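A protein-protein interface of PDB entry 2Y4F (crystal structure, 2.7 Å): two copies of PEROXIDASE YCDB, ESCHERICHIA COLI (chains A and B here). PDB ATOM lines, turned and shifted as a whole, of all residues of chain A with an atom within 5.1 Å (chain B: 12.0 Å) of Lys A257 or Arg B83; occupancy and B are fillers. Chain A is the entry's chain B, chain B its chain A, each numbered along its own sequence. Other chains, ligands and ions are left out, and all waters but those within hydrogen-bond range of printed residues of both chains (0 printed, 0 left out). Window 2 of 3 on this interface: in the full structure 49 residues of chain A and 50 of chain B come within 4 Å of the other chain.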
ATOM      1  N   PRO A 255     -21.104  16.241  -5.709  1.00  0.00           N
ATOM      2  CA  PRO A 255     -21.439  15.868  -7.078  1.00  0.00           C
ATOM      3  C   PRO A 255     -22.288  16.910  -7.772  1.00  0.00           C
ATOM      4  O   PRO A 255     -23.181  17.481  -7.140  1.00  0.00           O
ATOM      5  CB  PRO A 255     -22.259  14.601  -6.882  1.00  0.00           C
ATOM      6  CG  PRO A 255     -21.650  13.982  -5.690  1.00  0.00           C
ATOM      7  CD  PRO A 255     -21.192  15.078  -4.800  1.00  0.00           C
ATOM      8  N   LEU A 256     -22.036  17.146  -9.059  1.00  0.00           N
ATOM      9  CA  LEU A 256     -22.815  18.127  -9.797  1.00  0.00           C
ATOM     10  C   LEU A 256     -24.274  17.698  -9.827  1.00  0.00           C
ATOM     11  O   LEU A 256     -25.176  18.491  -9.548  1.00  0.00           O
ATOM     12  CB  LEU A 256     -22.258  18.315 -11.206  1.00  0.00           C
ATOM     13  CG  LEU A 256     -23.098  19.225 -12.113  1.00  0.00           C
ATOM     14  CD1 LEU A 256     -23.153  20.672 -11.636  1.00  0.00           C
ATOM     15  CD2 LEU A 256     -22.628  19.149 -13.572  1.00  0.00           C
ATOM     16  N   LYS A 257     -24.483  16.424 -10.155  1.00  0.00           N
ATOM     17  CA  LYS A 257     -25.793  15.779 -10.101  1.00  0.00           C
ATOM     18  C   LYS A 257     -26.490  16.139  -8.808  1.00  0.00           C
ATOM     19  O   LYS A 257     -27.660  16.489  -8.820  1.00  0.00           O
ATOM     20  CB  LYS A 257     -25.657  14.253 -10.234  1.00  0.00           C
ATOM     21  CG  LYS A 257     -26.960  13.453 -10.006  1.00  0.00           C
ATOM     22  CD  LYS A 257     -26.972  12.136 -10.775  1.00  0.00           C
ATOM     23  CE  LYS A 257     -26.399  10.988  -9.944  1.00  0.00           C
ATOM     24  NZ  LYS A 257     -27.471  10.110  -9.354  1.00  0.00           N
ATOM     25  N   GLU A 258     -25.766  16.070  -7.692  1.00  0.00           N
ATOM     26  CA  GLU A 258     -26.372  16.386  -6.397  1.00  0.00           C
ATOM     27  C   GLU A 258     -26.655  17.881  -6.225  1.00  0.00           C
ATOM     28  O   GLU A 258     -27.701  18.242  -5.682  1.00  0.00           O
ATOM     29  CB  GLU A 258     -25.548  15.832  -5.229  1.00  0.00           C
ATOM     30  CG  GLU A 258     -26.337  15.642  -3.924  1.00  0.00           C
ATOM     31  CD  GLU A 258     -25.457  15.178  -2.763  1.00  0.00           C
ATOM     32  OE1 GLU A 258     -24.442  14.474  -3.008  1.00  0.00           O
ATOM     33  OE2 GLU A 258     -25.780  15.517  -1.599  1.00  0.00           O
ATOM     34  N   GLN A 259     -25.747  18.739  -6.703  1.00  0.00           N
ATOM     35  CA  GLN A 259     -25.964  20.201  -6.649  1.00  0.00           C
ATOM     36  C   GLN A 259     -27.252  20.646  -7.375  1.00  0.00           C
ATOM     37  O   GLN A 259     -28.071  21.380  -6.813  1.00  0.00           O
ATOM     38  CB  GLN A 259     -24.751  20.971  -7.167  1.00  0.00           C
ATOM     39  CG  GLN A 259     -23.469  20.731  -6.367  1.00  0.00           C
ATOM     40  CD  GLN A 259     -22.275  21.546  -6.889  1.00  0.00           C
ATOM     41  OE1 GLN A 259     -22.412  22.356  -7.822  1.00  0.00           O
ATOM     42  NE2 GLN A 259     -21.105  21.340  -6.283  1.00  0.00           N
ATOM     43  N   GLN A 260     -27.447  20.165  -8.597  1.00  0.00           N
ATOM     44  CA  GLN A 260     -28.622  20.543  -9.377  1.00  0.00           C
ATOM     45  C   GLN A 260     -29.920  20.011  -8.739  1.00  0.00           C
ATOM     46  O   GLN A 260     -30.876  20.763  -8.500  1.00  0.00           O
ATOM     47  CB  GLN A 260     -28.454  20.120 -10.859  1.00  0.00           C
ATOM     48  CG  GLN A 260     -27.020  20.425 -11.457  1.00  0.00           C
ATOM     49  CD  GLN A 260     -26.979  20.692 -12.986  1.00  0.00           C
ATOM     50  OE1 GLN A 260     -27.910  21.232 -13.565  1.00  0.00           O
ATOM     51  NE2 GLN A 260     -25.880  20.343 -13.613  1.00  0.00           N
ATOM     52  N   THR A 261     -29.922  18.719  -8.432  1.00  0.00           N
ATOM     53  CA  THR A 261     -31.005  18.065  -7.688  1.00  0.00           C
ATOM     54  C   THR A 261     -31.485  18.890  -6.490  1.00  0.00           C
ATOM     55  O   THR A 261     -32.679  19.129  -6.337  1.00  0.00           O
ATOM     56  CB  THR A 261     -30.540  16.674  -7.203  1.00  0.00           C
ATOM     57  OG1 THR A 261     -30.186  15.871  -8.342  1.00  0.00           O
ATOM     58  CG2 THR A 261     -31.630  15.972  -6.394  1.00  0.00           C
ATOM     59  N   GLU B  78     -14.706  21.330 -18.193  1.00  0.00           N
ATOM     60  CA  GLU B  78     -16.010  20.712 -18.309  1.00  0.00           C
ATOM     61  C   GLU B  78     -15.998  19.393 -17.538  1.00  0.00           C
ATOM     62  O   GLU B  78     -14.984  18.683 -17.529  1.00  0.00           O
ATOM     63  CB  GLU B  78     -16.392  20.548 -19.793  1.00  0.00           C
ATOM     64  CG  GLU B  78     -17.864  20.162 -20.095  1.00  0.00           C
ATOM     65  CD  GLU B  78     -18.880  20.652 -19.052  1.00  0.00           C
ATOM     66  OE1 GLU B  78     -18.832  21.838 -18.651  1.00  0.00           O
ATOM     67  OE2 GLU B  78     -19.732  19.833 -18.633  1.00  0.00           O
ATOM     68  N   THR B  79     -17.115  19.106 -16.864  1.00  0.00           N
ATOM     69  CA  THR B  79     -17.292  17.896 -16.047  1.00  0.00           C
ATOM     70  C   THR B  79     -18.225  16.894 -16.750  1.00  0.00           C
ATOM     71  O   THR B  79     -19.449  16.951 -16.567  1.00  0.00           O
ATOM     72  CB  THR B  79     -17.855  18.250 -14.630  1.00  0.00           C
ATOM     73  OG1 THR B  79     -19.243  18.611 -14.719  1.00  0.00           O
ATOM     74  CG2 THR B  79     -17.103  19.409 -14.043  1.00  0.00           C
ATOM     75  N   PRO B  80     -17.654  15.962 -17.544  1.00  0.00           N
ATOM     76  CA  PRO B  80     -18.493  15.141 -18.444  1.00  0.00           C
ATOM     77  C   PRO B  80     -19.372  14.120 -17.704  1.00  0.00           C
ATOM     78  O   PRO B  80     -20.435  13.735 -18.205  1.00  0.00           O
ATOM     79  CB  PRO B  80     -17.472  14.434 -19.344  1.00  0.00           C
ATOM     80  CG  PRO B  80     -16.159  14.474 -18.590  1.00  0.00           C
ATOM     81  CD  PRO B  80     -16.270  15.456 -17.441  1.00  0.00           C
ATOM     82  N   ASN B  81     -18.915  13.709 -16.519  1.00  0.00           N
ATOM     83  CA  ASN B  81     -19.578  12.720 -15.677  1.00  0.00           C
ATOM     84  C   ASN B  81     -20.156  13.390 -14.408  1.00  0.00           C
ATOM     85  O   ASN B  81     -19.437  13.604 -13.434  1.00  0.00           O
ATOM     86  CB  ASN B  81     -18.570  11.596 -15.361  1.00  0.00           C
ATOM     87  CG  ASN B  81     -19.048  10.625 -14.283  1.00  0.00           C
ATOM     88  OD1 ASN B  81     -20.246  10.432 -14.064  1.00  0.00           O
ATOM     89  ND2 ASN B  81     -18.091   9.995 -13.610  1.00  0.00           N
ATOM     90  N   PRO B  82     -21.465  13.720 -14.427  1.00  0.00           N
ATOM     91  CA  PRO B  82     -22.155  14.458 -13.357  1.00  0.00           C
ATOM     92  C   PRO B  82     -22.101  13.809 -11.985  1.00  0.00           C
ATOM     93  O   PRO B  82     -22.366  14.480 -10.988  1.00  0.00           O
ATOM     94  CB  PRO B  82     -23.611  14.504 -13.833  1.00  0.00           C
ATOM     95  CG  PRO B  82     -23.545  14.318 -15.308  1.00  0.00           C
ATOM     96  CD  PRO B  82     -22.389  13.372 -15.526  1.00  0.00           C
ATOM     97  N   ARG B  83     -21.768  12.522 -11.921  1.00  0.00           N
ATOM     98  CA  ARG B  83     -21.673  11.822 -10.635  1.00  0.00           C
ATOM     99  C   ARG B  83     -20.472  12.299  -9.827  1.00  0.00           C
ATOM    100  O   ARG B  83     -20.239  11.843  -8.699  1.00  0.00           O
ATOM    101  CB  ARG B  83     -21.599  10.307 -10.841  1.00  0.00           C
ATOM    102  CG  ARG B  83     -22.952   9.615 -10.909  1.00  0.00           C
ATOM    103  CD  ARG B  83     -22.812   8.217 -11.472  1.00  0.00           C
ATOM    104  NE  ARG B  83     -22.734   8.193 -12.933  1.00  0.00           N
ATOM    105  CZ  ARG B  83     -23.787   8.234 -13.755  1.00  0.00           C
ATOM    106  NH1 ARG B  83     -25.034   8.329 -13.281  1.00  0.00           N
ATOM    107  NH2 ARG B  83     -23.592   8.191 -15.070  1.00  0.00           N
ATOM    108  N   LEU B  84     -19.719  13.221 -10.417  1.00  0.00           N
ATOM    109  CA  LEU B  84     -18.535  13.772  -9.794  1.00  0.00           C
ATOM    110  C   LEU B  84     -18.792  15.207  -9.323  1.00  0.00           C
ATOM    111  O   LEU B  84     -19.678  15.888  -9.858  1.00  0.00           O
ATOM    112  CB  LEU B  84     -17.366  13.768 -10.784  1.00  0.00           C
ATOM    113  CG  LEU B  84     -16.810  12.450 -11.314  1.00  0.00           C
ATOM    114  CD1 LEU B  84     -16.126  12.725 -12.637  1.00  0.00           C
ATOM    115  CD2 LEU B  84     -15.850  11.758 -10.324  1.00  0.00           C
ATOM    116  N   PRO B  85     -18.008  15.674  -8.329  1.00  0.00           N
ATOM    117  CA  PRO B  85     -18.045  17.093  -8.040  1.00  0.00           C
ATOM    118  C   PRO B  85     -17.574  17.849  -9.296  1.00  0.00           C
ATOM    119  O   PRO B  85     -16.678  17.361  -9.995  1.00  0.00           O
ATOM    120  CB  PRO B  85     -17.017  17.247  -6.912  1.00  0.00           C
ATOM    121  CG  PRO B  85     -16.687  15.874  -6.460  1.00  0.00           C
ATOM    122  CD  PRO B  85     -16.910  14.997  -7.611  1.00  0.00           C
ATOM    123  N   PRO B  86     -18.193  19.008  -9.606  1.00  0.00           N
ATOM    124  CA  PRO B  86     -17.749  19.815 -10.755  1.00  0.00           C
ATOM    125  C   PRO B  86     -16.289  20.230 -10.607  1.00  0.00           C
ATOM    126  O   PRO B  86     -15.864  20.585  -9.502  1.00  0.00           O
ATOM    127  CB  PRO B  86     -18.647  21.051 -10.706  1.00  0.00           C
ATOM    128  CG  PRO B  86     -19.804  20.687  -9.840  1.00  0.00           C
ATOM    129  CD  PRO B  86     -19.344  19.606  -8.902  1.00  0.00           C
ATOM    130  N   LEU B  87     -15.533  20.173 -11.707  1.00  0.00           N
ATOM    131  CA  LEU B  87     -14.081  20.425 -11.697  1.00  0.00           C
ATOM    132  C   LEU B  87     -13.832  21.907 -11.500  1.00  0.00           C
ATOM    133  O   LEU B  87     -12.793  22.312 -10.986  1.00  0.00           O
ATOM    134  CB  LEU B  87     -13.415  19.933 -12.993  1.00  0.00           C
ATOM    135  CG  LEU B  87     -13.854  18.612 -13.651  1.00  0.00           C
ATOM    136  CD1 LEU B  87     -13.048  18.316 -14.895  1.00  0.00           C
ATOM    137  CD2 LEU B  87     -13.782  17.424 -12.693  1.00  0.00           C
ATOM    138  N   ASP B  88     -14.806  22.705 -11.915  1.00  0.00           N
ATOM    139  CA  ASP B  88     -14.816  24.122 -11.631  1.00  0.00           C
ATOM    140  C   ASP B  88     -16.004  24.487 -10.718  1.00  0.00           C
ATOM    141  O   ASP B  88     -17.058  23.833 -10.754  1.00  0.00           O
ATOM    142  CB  ASP B  88     -14.891  24.918 -12.935  1.00  0.00           C
ATOM    143  CG  ASP B  88     -14.548  26.373 -12.743  1.00  0.00           C
ATOM    144  OD1 ASP B  88     -13.328  26.690 -12.715  1.00  0.00           O
ATOM    145  OD2 ASP B  88     -15.499  27.187 -12.630  1.00  0.00           O
ATOM    146  N   SER B  89     -15.814  25.533  -9.910  1.00  0.00           N
ATOM    147  CA  SER B  89     -16.849  26.054  -9.013  1.00  0.00           C
ATOM    148  C   SER B  89     -17.975  26.751  -9.761  1.00  0.00           C
ATOM    149  O   SER B  89     -19.041  26.957  -9.211  1.00  0.00           O
ATOM    150  CB  SER B  89     -16.233  27.055  -8.038  1.00  0.00           C
ATOM    151  OG  SER B  89     -15.607  28.116  -8.747  1.00  0.00           O
ATOM    152  N   LYS B 167      -9.792  22.877  -3.591  1.00  0.00           N
ATOM    153  CA  LYS B 167     -10.409  21.676  -4.122  1.00  0.00           C
ATOM    154  C   LYS B 167      -9.333  20.675  -4.491  1.00  0.00           C
ATOM    155  O   LYS B 167      -9.476  19.490  -4.205  1.00  0.00           O
ATOM    156  CB  LYS B 167     -11.255  21.992  -5.345  1.00  0.00           C
ATOM    157  CG  LYS B 167     -12.221  20.889  -5.682  1.00  0.00           C
ATOM    158  CD  LYS B 167     -12.547  20.805  -7.170  1.00  0.00           C
ATOM    159  CE  LYS B 167     -12.915  19.353  -7.553  1.00  0.00           C
ATOM    160  NZ  LYS B 167     -13.764  19.297  -8.763  1.00  0.00           N
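N of Lys A257 sits at hydrogen-bond distance from O of Pro B82 (3.0 Å).
The backbone carbonyl oxygen (O) of Leu B84 is in hydrogen-bond range of the backbone NH (N) of Leu A256 (2.8 Å).
O of Pro B82 sits at hydrogen-bond distance from N of Leu A256 (3.3 Å).
O of Pro B86 is in hydrogen-bond range of NZ of Lys B167, 2.6 Å away.
The backbone carbonyl oxygen of Lys A257 is in hydrogen-bond range of the side-chain hydroxyl of Thr A261 (2.6 Å).
The backbone NH (N) of Arg B83 lies close to the side-chain amide oxygen (OD1) of Asn B81 (3.4 Å).
Pro A255 touches Arg B83 (CB to O, 3.9 Å).
Leu B84 touches Pro A255 (O to CA, 3.3 Å).
Pro B85 touches Pro A255.
Thr B79 touches Leu A256 (OG1 to CD2, 3.6 Å).
CD of Pro B86 touches N of Leu A256, 3.7 Å away.
Arg B83 touches Lys A257.
Gln A259 touches Pro B86 (NE2 to CD, 3.6 Å).
Arg B83 touches two residues of chain A.
Pro A255 touches three residues of chain B.
Leu A256 touches just these residues of chain B: Thr B79 (3.6 Å), Pro B82 (3.3 Å), Leu B84 (2.8 Å) and Pro B86 (3.7 Å).
No residue of chain B comes within 4 Å of Glu A258.
Of the printed residues of chain B, Gln A259 touches Pro B86 (3.6 Å).
No residue of chain B comes within 4 Å of Thr A261.
Of the printed residues of chain A, Leu B84 touches Pro A255 (3.3 Å) and Leu A256 (2.8 Å).
Of the printed residues of chain A, Pro B86 touches Leu A256 and Gln A259.
The nearest residue of chain B that does not touch Lys A257 is Leu B84 (4.8 Å).
The nearest printed residue of chain A that does not touch Arg B83 is Leu A256 (5.2 Å).
The nearest printed residue of chain A that does not touch Leu B84 is Lys A257 (4.8 Å).
Of the 13 printed residues of chain B, 6 touch a printed residue of chain A.
Hydrophobic or aromatic side chains of chain B that line the printed part of chain A: Pro B86.
Hydrophobic or aromatic side chains of chain A within 4 Å of the printed part of chain B: Pro A255 and Leu A256.
Among the printed residues, 10 pairs touch across the chains.
No position is printed for both chains.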
